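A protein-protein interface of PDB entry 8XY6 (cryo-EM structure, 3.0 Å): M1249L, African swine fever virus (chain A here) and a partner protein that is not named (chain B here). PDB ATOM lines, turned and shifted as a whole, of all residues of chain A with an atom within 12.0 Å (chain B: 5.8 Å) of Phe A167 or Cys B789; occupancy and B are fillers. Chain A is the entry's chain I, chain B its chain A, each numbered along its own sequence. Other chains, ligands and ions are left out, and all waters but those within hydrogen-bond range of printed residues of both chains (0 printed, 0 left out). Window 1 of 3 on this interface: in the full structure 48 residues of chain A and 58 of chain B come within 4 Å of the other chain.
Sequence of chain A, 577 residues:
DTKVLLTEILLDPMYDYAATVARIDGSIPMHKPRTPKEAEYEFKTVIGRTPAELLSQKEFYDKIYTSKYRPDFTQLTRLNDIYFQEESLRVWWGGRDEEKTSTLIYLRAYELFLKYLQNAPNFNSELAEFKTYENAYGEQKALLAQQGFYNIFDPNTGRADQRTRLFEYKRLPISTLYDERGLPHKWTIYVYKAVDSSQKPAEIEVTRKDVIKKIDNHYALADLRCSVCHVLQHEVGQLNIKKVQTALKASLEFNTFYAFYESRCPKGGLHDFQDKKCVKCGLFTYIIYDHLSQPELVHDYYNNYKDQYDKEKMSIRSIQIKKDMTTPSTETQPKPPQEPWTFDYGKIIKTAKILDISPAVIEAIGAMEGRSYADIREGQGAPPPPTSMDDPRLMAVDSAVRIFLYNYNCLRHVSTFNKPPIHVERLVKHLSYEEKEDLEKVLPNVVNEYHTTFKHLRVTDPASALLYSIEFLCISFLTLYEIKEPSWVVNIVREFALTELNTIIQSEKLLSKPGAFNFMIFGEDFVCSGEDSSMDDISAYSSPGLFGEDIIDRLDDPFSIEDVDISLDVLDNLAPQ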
ATOM      1  N   GLN A 162      23.334   5.934  -4.024  1.00  0.00           N
ATOM      2  CA  GLN A 162      23.231   7.023  -3.066  1.00  0.00           C
ATOM      3  C   GLN A 162      23.832   8.320  -3.591  1.00  0.00           C
ATOM      4  O   GLN A 162      23.917   9.300  -2.844  1.00  0.00           O
ATOM      5  CB  GLN A 162      23.908   6.634  -1.750  1.00  0.00           C
ATOM      6  CG  GLN A 162      23.183   7.098  -0.496  1.00  0.00           C
ATOM      7  CD  GLN A 162      21.942   6.282  -0.182  1.00  0.00           C
ATOM      8  OE1 GLN A 162      21.239   5.818  -1.076  1.00  0.00           O
ATOM      9  NE2 GLN A 162      21.669   6.107   1.104  1.00  0.00           N
ATOM     10  N   ARG A 163      24.260   8.349  -4.851  1.00  0.00           N
ATOM     11  CA  ARG A 163      24.770   9.580  -5.436  1.00  0.00           C
ATOM     12  C   ARG A 163      23.614  10.515  -5.754  1.00  0.00           C
ATOM     13  O   ARG A 163      22.620  10.105  -6.360  1.00  0.00           O
ATOM     14  CB  ARG A 163      25.567   9.287  -6.704  1.00  0.00           C
ATOM     15  CG  ARG A 163      26.698   8.304  -6.523  1.00  0.00           C
ATOM     16  CD  ARG A 163      27.125   7.733  -7.861  1.00  0.00           C
ATOM     17  NE  ARG A 163      26.047   6.989  -8.500  1.00  0.00           N
ATOM     18  CZ  ARG A 163      26.142   6.412  -9.689  1.00  0.00           C
ATOM     19  NH1 ARG A 163      27.252   6.485 -10.404  1.00  0.00           N
ATOM     20  NH2 ARG A 163      25.099   5.747 -10.172  1.00  0.00           N
ATOM     21  N   THR A 164      23.744  11.774  -5.348  1.00  0.00           N
ATOM     22  CA  THR A 164      22.703  12.762  -5.564  1.00  0.00           C
ATOM     23  C   THR A 164      23.334  14.094  -5.934  1.00  0.00           C
ATOM     24  O   THR A 164      24.486  14.370  -5.594  1.00  0.00           O
ATOM     25  CB  THR A 164      21.824  12.939  -4.324  1.00  0.00           C
ATOM     26  OG1 THR A 164      22.644  12.924  -3.150  1.00  0.00           O
ATOM     27  CG2 THR A 164      20.796  11.832  -4.234  1.00  0.00           C
ATOM     28  N   ARG A 165      22.560  14.915  -6.634  1.00  0.00           N
ATOM     29  CA  ARG A 165      22.966  16.262  -7.003  1.00  0.00           C
ATOM     30  C   ARG A 165      22.468  17.309  -6.018  1.00  0.00           C
ATOM     31  O   ARG A 165      22.306  18.471  -6.398  1.00  0.00           O
ATOM     32  CB  ARG A 165      22.458  16.592  -8.407  1.00  0.00           C
ATOM     33  CG  ARG A 165      23.423  16.243  -9.521  1.00  0.00           C
ATOM     34  CD  ARG A 165      24.256  17.445  -9.913  1.00  0.00           C
ATOM     35  NE  ARG A 165      24.597  17.433 -11.331  1.00  0.00           N
ATOM     36  CZ  ARG A 165      23.740  17.678 -12.311  1.00  0.00           C
ATOM     37  NH1 ARG A 165      22.471  17.959 -12.068  1.00  0.00           N
ATOM     38  NH2 ARG A 165      24.169  17.642 -13.569  1.00  0.00           N
ATOM     39  N   LEU A 166      22.217  16.923  -4.772  1.00  0.00           N
ATOM     40  CA  LEU A 166      21.649  17.843  -3.803  1.00  0.00           C
ATOM     41  C   LEU A 166      22.658  18.916  -3.416  1.00  0.00           C
ATOM     42  O   LEU A 166      23.870  18.769  -3.586  1.00  0.00           O
ATOM     43  CB  LEU A 166      21.184  17.091  -2.558  1.00  0.00           C
ATOM     44  CG  LEU A 166      19.722  16.650  -2.515  1.00  0.00           C
ATOM     45  CD1 LEU A 166      19.435  15.632  -3.594  1.00  0.00           C
ATOM     46  CD2 LEU A 166      19.389  16.083  -1.151  1.00  0.00           C
ATOM     47  N   PHE A 167      22.129  20.014  -2.891  1.00  0.00           N
ATOM     48  CA  PHE A 167      22.947  21.146  -2.492  1.00  0.00           C
ATOM     49  C   PHE A 167      23.779  20.814  -1.257  1.00  0.00           C
ATOM     50  O   PHE A 167      23.302  20.171  -0.321  1.00  0.00           O
ATOM     51  CB  PHE A 167      22.044  22.345  -2.222  1.00  0.00           C
ATOM     52  CG  PHE A 167      22.748  23.518  -1.626  1.00  0.00           C
ATOM     53  CD1 PHE A 167      23.446  24.394  -2.424  1.00  0.00           C
ATOM     54  CD2 PHE A 167      22.699  23.752  -0.268  1.00  0.00           C
ATOM     55  CE1 PHE A 167      24.085  25.472  -1.878  1.00  0.00           C
ATOM     56  CE2 PHE A 167      23.336  24.831   0.280  1.00  0.00           C
ATOM     57  CZ  PHE A 167      24.028  25.692  -0.525  1.00  0.00           C
ATOM     58  N   GLU A 168      25.031  21.264  -1.257  1.00  0.00           N
ATOM     59  CA  GLU A 168      25.916  21.142  -0.108  1.00  0.00           C
ATOM     60  C   GLU A 168      26.357  22.536   0.319  1.00  0.00           C
ATOM     61  O   GLU A 168      26.536  23.420  -0.522  1.00  0.00           O
ATOM     62  CB  GLU A 168      27.130  20.264  -0.428  1.00  0.00           C
ATOM     63  CG  GLU A 168      27.979  19.910   0.787  1.00  0.00           C
ATOM     64  CD  GLU A 168      29.281  19.225   0.419  1.00  0.00           C
ATOM     65  OE1 GLU A 168      29.964  19.698  -0.513  1.00  0.00           O
ATOM     66  OE2 GLU A 168      29.626  18.216   1.067  1.00  0.00           O
ATOM     67  N   TYR A 169      26.539  22.729   1.628  1.00  0.00           N
ATOM     68  CA  TYR A 169      26.646  24.082   2.167  1.00  0.00           C
ATOM     69  C   TYR A 169      27.913  24.784   1.688  1.00  0.00           C
ATOM     70  O   TYR A 169      27.838  25.838   1.051  1.00  0.00           O
ATOM     71  CB  TYR A 169      26.585  24.052   3.691  1.00  0.00           C
ATOM     72  CG  TYR A 169      26.865  25.398   4.305  1.00  0.00           C
ATOM     73  CD1 TYR A 169      26.071  26.491   4.003  1.00  0.00           C
ATOM     74  CD2 TYR A 169      27.925  25.579   5.179  1.00  0.00           C
ATOM     75  CE1 TYR A 169      26.322  27.723   4.552  1.00  0.00           C
ATOM     76  CE2 TYR A 169      28.185  26.811   5.735  1.00  0.00           C
ATOM     77  CZ  TYR A 169      27.379  27.880   5.418  1.00  0.00           C
ATOM     78  OH  TYR A 169      27.634  29.114   5.970  1.00  0.00           O
ATOM     79  N   LYS A 170      29.083  24.236   2.005  1.00  0.00           N
ATOM     80  CA  LYS A 170      30.357  24.718   1.463  1.00  0.00           C
ATOM     81  C   LYS A 170      30.547  26.221   1.690  1.00  0.00           C
ATOM     82  O   LYS A 170      30.475  27.030   0.769  1.00  0.00           O
ATOM     83  CB  LYS A 170      30.482  24.390  -0.027  1.00  0.00           C
ATOM     84  CG  LYS A 170      30.324  22.928  -0.373  1.00  0.00           C
ATOM     85  CD  LYS A 170      30.869  22.644  -1.759  1.00  0.00           C
ATOM     86  CE  LYS A 170      30.366  23.655  -2.776  1.00  0.00           C
ATOM     87  NZ  LYS A 170      28.881  23.773  -2.766  1.00  0.00           N
ATOM     88  N   ARG A 171      30.739  26.575   2.959  1.00  0.00           N
ATOM     89  CA  ARG A 171      31.110  27.934   3.342  1.00  0.00           C
ATOM     90  C   ARG A 171      32.199  28.491   2.429  1.00  0.00           C
ATOM     91  O   ARG A 171      33.167  27.800   2.105  1.00  0.00           O
ATOM     92  CB  ARG A 171      31.597  27.933   4.790  1.00  0.00           C
ATOM     93  CG  ARG A 171      32.508  29.085   5.156  1.00  0.00           C
ATOM     94  CD  ARG A 171      32.790  29.122   6.655  1.00  0.00           C
ATOM     95  NE  ARG A 171      31.764  28.447   7.443  1.00  0.00           N
ATOM     96  CZ  ARG A 171      30.560  28.945   7.695  1.00  0.00           C
ATOM     97  NH1 ARG A 171      30.179  30.109   7.201  1.00  0.00           N
ATOM     98  NH2 ARG A 171      29.712  28.246   8.444  1.00  0.00           N
ATOM     99  N   LEU A 172      32.035  29.747   2.018  1.00  0.00           N
ATOM    100  CA  LEU A 172      32.947  30.403   1.090  1.00  0.00           C
ATOM    101  C   LEU A 172      33.691  31.557   1.748  1.00  0.00           C
ATOM    102  O   LEU A 172      33.264  32.080   2.782  1.00  0.00           O
ATOM    103  CB  LEU A 172      32.197  30.945  -0.132  1.00  0.00           C
ATOM    104  CG  LEU A 172      31.184  30.085  -0.866  1.00  0.00           C
ATOM    105  CD1 LEU A 172      30.557  30.936  -1.941  1.00  0.00           C
ATOM    106  CD2 LEU A 172      31.857  28.875  -1.469  1.00  0.00           C
ATOM    107  N   HIS B 663      25.724  23.160 -12.425  1.00  0.00           N
ATOM    108  CA  HIS B 663      25.283  22.811 -11.082  1.00  0.00           C
ATOM    109  C   HIS B 663      26.250  23.340 -10.032  1.00  0.00           C
ATOM    110  O   HIS B 663      25.823  23.839  -8.986  1.00  0.00           O
ATOM    111  CB  HIS B 663      25.118  21.302 -10.948  1.00  0.00           C
ATOM    112  CG  HIS B 663      24.627  20.874  -9.604  1.00  0.00           C
ATOM    113  ND1 HIS B 663      25.467  20.389  -8.625  1.00  0.00           N
ATOM    114  CD2 HIS B 663      23.383  20.868  -9.070  1.00  0.00           C
ATOM    115  CE1 HIS B 663      24.761  20.099  -7.547  1.00  0.00           C
ATOM    116  NE2 HIS B 663      23.494  20.380  -7.791  1.00  0.00           N
ATOM    117  N   VAL B 666      25.524  27.028  -9.738  1.00  0.00           N
ATOM    118  CA  VAL B 666      24.325  27.249  -8.932  1.00  0.00           C
ATOM    119  C   VAL B 666      24.645  27.071  -7.456  1.00  0.00           C
ATOM    120  O   VAL B 666      24.202  27.856  -6.603  1.00  0.00           O
ATOM    121  CB  VAL B 666      23.199  26.298  -9.377  1.00  0.00           C
ATOM    122  CG1 VAL B 666      22.142  26.194  -8.304  1.00  0.00           C
ATOM    123  CG2 VAL B 666      22.584  26.774 -10.666  1.00  0.00           C
ATOM    124  N   GLN B 667      25.413  26.029  -7.131  1.00  0.00           N
ATOM    125  CA  GLN B 667      25.848  25.828  -5.757  1.00  0.00           C
ATOM    126  C   GLN B 667      26.642  27.022  -5.259  1.00  0.00           C
ATOM    127  O   GLN B 667      26.470  27.449  -4.117  1.00  0.00           O
ATOM    128  CB  GLN B 667      26.686  24.557  -5.646  1.00  0.00           C
ATOM    129  CG  GLN B 667      25.880  23.286  -5.497  1.00  0.00           C
ATOM    130  CD  GLN B 667      26.651  22.201  -4.781  1.00  0.00           C
ATOM    131  OE1 GLN B 667      27.791  22.404  -4.372  1.00  0.00           O
ATOM    132  NE2 GLN B 667      26.033  21.038  -4.629  1.00  0.00           N
ATOM    133  N   ILE B 670      24.228  29.967  -4.518  1.00  0.00           N
ATOM    134  CA  ILE B 670      23.476  29.746  -3.288  1.00  0.00           C
ATOM    135  C   ILE B 670      24.396  29.814  -2.077  1.00  0.00           C
ATOM    136  O   ILE B 670      23.989  30.278  -1.007  1.00  0.00           O
ATOM    137  CB  ILE B 670      22.708  28.417  -3.356  1.00  0.00           C
ATOM    138  CG1 ILE B 670      21.716  28.446  -4.516  1.00  0.00           C
ATOM    139  CG2 ILE B 670      21.952  28.183  -2.074  1.00  0.00           C
ATOM    140  CD1 ILE B 670      20.746  27.295  -4.516  1.00  0.00           C
ATOM    141  N   ASN B 671      25.646  29.370  -2.218  1.00  0.00           N
ATOM    142  CA  ASN B 671      26.603  29.491  -1.125  1.00  0.00           C
ATOM    143  C   ASN B 671      26.883  30.947  -0.800  1.00  0.00           C
ATOM    144  O   ASN B 671      27.057  31.301   0.366  1.00  0.00           O
ATOM    145  CB  ASN B 671      27.905  28.778  -1.470  1.00  0.00           C
ATOM    146  CG  ASN B 671      27.754  27.292  -1.523  1.00  0.00           C
ATOM    147  OD1 ASN B 671      26.720  26.757  -1.153  1.00  0.00           O
ATOM    148  ND2 ASN B 671      28.790  26.605  -1.982  1.00  0.00           N
ATOM    149  N   LEU B 674      23.909  32.180   1.191  1.00  0.00           N
ATOM    150  CA  LEU B 674      24.005  31.696   2.560  1.00  0.00           C
ATOM    151  C   LEU B 674      25.166  32.337   3.301  1.00  0.00           C
ATOM    152  O   LEU B 674      25.112  32.476   4.523  1.00  0.00           O
ATOM    153  CB  LEU B 674      24.145  30.179   2.568  1.00  0.00           C
ATOM    154  CG  LEU B 674      22.918  29.431   2.064  1.00  0.00           C
ATOM    155  CD1 LEU B 674      23.141  27.942   2.157  1.00  0.00           C
ATOM    156  CD2 LEU B 674      21.716  29.839   2.874  1.00  0.00           C
ATOM    157  N   PHE B 711      17.484  35.500  -4.930  1.00  0.00           N
ATOM    158  CA  PHE B 711      18.270  35.001  -6.051  1.00  0.00           C
ATOM    159  C   PHE B 711      18.741  36.156  -6.924  1.00  0.00           C
ATOM    160  O   PHE B 711      17.910  36.949  -7.383  1.00  0.00           O
ATOM    161  CB  PHE B 711      17.438  34.032  -6.877  1.00  0.00           C
ATOM    162  CG  PHE B 711      17.552  32.610  -6.432  1.00  0.00           C
ATOM    163  CD1 PHE B 711      18.731  32.132  -5.897  1.00  0.00           C
ATOM    164  CD2 PHE B 711      16.477  31.750  -6.545  1.00  0.00           C
ATOM    165  CE1 PHE B 711      18.838  30.825  -5.487  1.00  0.00           C
ATOM    166  CE2 PHE B 711      16.580  30.442  -6.137  1.00  0.00           C
ATOM    167  CZ  PHE B 711      17.760  29.979  -5.607  1.00  0.00           C
ATOM    168  N   ALA B 750      17.460  25.638 -10.872  1.00  0.00           N
ATOM    169  CA  ALA B 750      18.493  26.139  -9.971  1.00  0.00           C
ATOM    170  C   ALA B 750      18.136  25.950  -8.498  1.00  0.00           C
ATOM    171  O   ALA B 750      18.862  25.280  -7.760  1.00  0.00           O
ATOM    172  CB  ALA B 750      18.766  27.616 -10.265  1.00  0.00           C
ATOM    173  N   GLY B 751      17.034  26.546  -8.053  1.00  0.00           N
ATOM    174  CA  GLY B 751      16.635  26.426  -6.663  1.00  0.00           C
ATOM    175  C   GLY B 751      15.339  27.137  -6.340  1.00  0.00           C
ATOM    176  O   GLY B 751      14.924  28.037  -7.073  1.00  0.00           O
ATOM    177  N   ILE B 752      14.690  26.749  -5.243  1.00  0.00           N
ATOM    178  CA  ILE B 752      13.409  27.350  -4.888  1.00  0.00           C
ATOM    179  C   ILE B 752      13.609  28.670  -4.159  1.00  0.00           C
ATOM    180  O   ILE B 752      12.837  29.615  -4.341  1.00  0.00           O
ATOM    181  CB  ILE B 752      12.570  26.372  -4.052  1.00  0.00           C
ATOM    182  CG1 ILE B 752      12.612  24.976  -4.660  1.00  0.00           C
ATOM    183  CG2 ILE B 752      11.140  26.851  -3.956  1.00  0.00           C
ATOM    184  CD1 ILE B 752      12.089  24.920  -6.054  1.00  0.00           C
ATOM    185  N   GLY B 753      14.631  28.758  -3.320  1.00  0.00           N
ATOM    186  CA  GLY B 753      14.858  29.973  -2.574  1.00  0.00           C
ATOM    187  C   GLY B 753      13.960  30.077  -1.354  1.00  0.00           C
ATOM    188  O   GLY B 753      13.333  29.111  -0.915  1.00  0.00           O
ATOM    189  N   GLN B 783      18.265  27.834   6.359  1.00  0.00           N
ATOM    190  CA  GLN B 783      17.410  26.729   5.940  1.00  0.00           C
ATOM    191  C   GLN B 783      16.339  26.422   6.974  1.00  0.00           C
ATOM    192  O   GLN B 783      15.278  25.891   6.629  1.00  0.00           O
ATOM    193  CB  GLN B 783      18.256  25.486   5.678  1.00  0.00           C
ATOM    194  CG  GLN B 783      19.283  25.660   4.588  1.00  0.00           C
ATOM    195  CD  GLN B 783      20.636  26.051   5.127  1.00  0.00           C
ATOM    196  OE1 GLN B 783      20.825  27.167   5.604  1.00  0.00           O
ATOM    197  NE2 GLN B 783      21.590  25.134   5.056  1.00  0.00           N
ATOM    198  N   PHE B 787      14.258  28.586   3.848  1.00  0.00           N
ATOM    199  CA  PHE B 787      15.094  28.731   2.663  1.00  0.00           C
ATOM    200  C   PHE B 787      15.331  27.357   2.057  1.00  0.00           C
ATOM    201  O   PHE B 787      15.996  26.510   2.660  1.00  0.00           O
ATOM    202  CB  PHE B 787      16.417  29.408   2.999  1.00  0.00           C
ATOM    203  CG  PHE B 787      17.269  29.680   1.797  1.00  0.00           C
ATOM    204  CD1 PHE B 787      16.855  30.572   0.833  1.00  0.00           C
ATOM    205  CD2 PHE B 787      18.480  29.040   1.627  1.00  0.00           C
ATOM    206  CE1 PHE B 787      17.632  30.824  -0.273  1.00  0.00           C
ATOM    207  CE2 PHE B 787      19.258  29.289   0.521  1.00  0.00           C
ATOM    208  CZ  PHE B 787      18.834  30.182  -0.427  1.00  0.00           C
ATOM    209  N   ILE B 788      14.789  27.136   0.868  1.00  0.00           N
ATOM    210  CA  ILE B 788      14.957  25.876   0.158  1.00  0.00           C
ATOM    211  C   ILE B 788      16.130  26.045  -0.795  1.00  0.00           C
ATOM    212  O   ILE B 788      16.108  26.910  -1.672  1.00  0.00           O
ATOM    213  CB  ILE B 788      13.682  25.481  -0.592  1.00  0.00           C
ATOM    214  CG1 ILE B 788      12.514  25.343   0.379  1.00  0.00           C
ATOM    215  CG2 ILE B 788      13.896  24.187  -1.335  1.00  0.00           C
ATOM    216  CD1 ILE B 788      11.262  24.822  -0.266  1.00  0.00           C
ATOM    217  N   CYS B 789      17.161  25.224  -0.620  1.00  0.00           N
ATOM    218  CA  CYS B 789      18.343  25.350  -1.461  1.00  0.00           C
ATOM    219  C   CYS B 789      18.253  24.463  -2.694  1.00  0.00           C
ATOM    220  O   CYS B 789      18.750  24.828  -3.763  1.00  0.00           O
ATOM    221  CB  CYS B 789      19.592  25.008  -0.656  1.00  0.00           C
ATOM    222  SG  CYS B 789      19.490  25.398   1.092  1.00  0.00           S
ATOM    223  N   ASN B 790      17.637  23.296  -2.562  1.00  0.00           N
ATOM    224  CA  ASN B 790      17.554  22.360  -3.668  1.00  0.00           C
ATOM    225  C   ASN B 790      16.502  22.802  -4.671  1.00  0.00           C
ATOM    226  O   ASN B 790      15.474  23.376  -4.313  1.00  0.00           O
ATOM    227  CB  ASN B 790      17.227  20.959  -3.158  1.00  0.00           C
ATOM    228  CG  ASN B 790      18.364  20.348  -2.379  1.00  0.00           C
ATOM    229  OD1 ASN B 790      19.378  19.953  -2.948  1.00  0.00           O
ATOM    230  ND2 ASN B 790      18.209  20.277  -1.064  1.00  0.00           N
ATOM    231  N   SER B 791      16.778  22.535  -5.942  1.00  0.00           N
ATOM    232  CA  SER B 791      15.803  22.755  -6.994  1.00  0.00           C
ATOM    233  C   SER B 791      14.815  21.598  -7.033  1.00  0.00           C
ATOM    234  O   SER B 791      14.998  20.568  -6.383  1.00  0.00           O
ATOM    235  CB  SER B 791      16.497  22.901  -8.343  1.00  0.00           C
ATOM    236  OG  SER B 791      17.311  21.776  -8.611  1.00  0.00           O
ATOM    237  N   ALA B 794      16.449  18.580  -8.581  1.00  0.00           N
ATOM    238  CA  ALA B 794      17.400  17.943  -7.682  1.00  0.00           C
ATOM    239  C   ALA B 794      16.718  17.160  -6.573  1.00  0.00           C
ATOM    240  O   ALA B 794      17.337  16.262  -5.997  1.00  0.00           O
ATOM    241  CB  ALA B 794      18.332  18.990  -7.074  1.00  0.00           C
ATOM    242  N   GLU B 800      12.680  20.704   3.621  1.00  0.00           N
ATOM    243  CA  GLU B 800      12.403  21.580   2.490  1.00  0.00           C
ATOM    244  C   GLU B 800      11.043  21.275   1.885  1.00  0.00           C
ATOM    245  O   GLU B 800      10.284  22.190   1.554  1.00  0.00           O
ATOM    246  CB  GLU B 800      13.495  21.443   1.435  1.00  0.00           C
ATOM    247  CG  GLU B 800      14.826  22.008   1.843  1.00  0.00           C
ATOM    248  CD  GLU B 800      15.964  21.364   1.094  1.00  0.00           C
ATOM    249  OE1 GLU B 800      15.802  21.102  -0.114  1.00  0.00           O
ATOM    250  OE2 GLU B 800      17.021  21.116   1.708  1.00  0.00           O
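Of chain B, only Gln B667, Ile B670, Asn B671, Leu B674, Cys B789 and Asn B790 come within 4 Å of Phe A167.
Of chain A, only Phe A167 (3.4 Å) comes within 4 Å of Cys B789.
Asn B671 touches just these residues of chain A: Phe A167 (3.0 Å), Glu A168 (3.4 Å), Tyr A169 (2.6 Å), Lys A170 (2.9 Å) and Leu A172 (3.5 Å).
No residue of chain A comes within 4 Å of Ala B750.
Gly B751 touches none of the printed residues of chain A.
No residue of chain A comes within 4 Å of Gly B753.
No residue of chain A comes within 4 Å of Gln B783.
Phe B787 touches none of the printed residues of chain A.
No residue of chain A comes within 4 Å of Ile B788.
Of chain A, only Leu A166 (3.2 Å) and Phe A167 (2.8 Å) come within 4 Å of Asn B790.
No residue of chain A comes within 4 Å of Ser B791.
No residue of chain A comes within 4 Å of Glu B800.
Printed residues of chain A within 4 Å of His B663: Arg A165 (2.6 Å).
Printed residues of chain A within 4 Å of Leu B674: Phe A167 (3.6 Å) and Tyr A169 (3.8 Å).
Gln A162 touches none of the printed residues of chain B.
The nearest residue of chain A that does not touch Cys B789 is Glu A168 (6.6 Å).
O of Gln B667 sits close to OD1 of Asn B671.
The backbone carbonyl oxygen (O) of Glu A168 sits at hydrogen-bond distance from the side-chain amino group (NZ) of Lys A170, at 3.3 Å.
NH1 of Arg A171 sits at hydrogen-bond distance from OH of Tyr A169 (3.0 Å).
OG of Ser B791 is in hydrogen-bond range of N of Ala B794.
OE1 of Glu B800 sits at hydrogen-bond distance from ND2 of Asn B790 (2.7 Å).
Printed residues of chain A that touch a printed residue of chain B: Arg A165, Leu A166, Phe A167, Glu A168, Tyr A169, Lys A170 and Leu A172.
Of the 19 printed residues of chain B, 8 touch a printed residue of chain A.
The side-chain amide oxygen (OD1) of Asn B671 sits close to the backbone carbonyl oxygen (O) of Tyr A169, 2.6 Å away.
The side-chain amide oxygen (OE1) of Gln B667 lies close to the side-chain amino group (NZ) of Lys A170 (2.4 Å).
The side-chain amide nitrogen of Asn B671 sits close to the side-chain amino group of Lys A170 (2.9 Å).
The backbone NH (N) of Phe A167 sits at hydrogen-bond distance from the side-chain amide oxygen (OD1) of Asn B790 (2.8 Å).
The backbone carbonyl oxygen of Glu A168 lies close to the side-chain amide oxygen of Asn B671, 3.4 Å away.
O of Arg A165 lies within hydrogen-bond range of NE2 of His B663, 2.6 Å away.
The backbone carbonyl oxygen (O) of Leu A166 sits at hydrogen-bond distance from the side-chain amide nitrogen (NE2) of Gln B667, at 3.3 Å.
Asn B790 touches Leu A166 (OD1 to CA, 3.2 Å).
Leu A166 touches Ala B794.
Phe A167 touches Gln B667.
Ile B670 touches Phe A167.
Asn B671 touches Phe A167 (OD1 to CZ, 3.0 Å).
Phe A167 touches Leu B674 (CZ to CD1, 3.6 Å).
Cys B789 touches Phe A167 (CB to CD2, 3.4 Å).
Gln B667 touches Glu A168.
Tyr A169 touches Leu B674 (CD1 to CD1, 3.8 Å).
CD1 of Leu A172 touches CB of Asn B671, 3.5 Å away.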
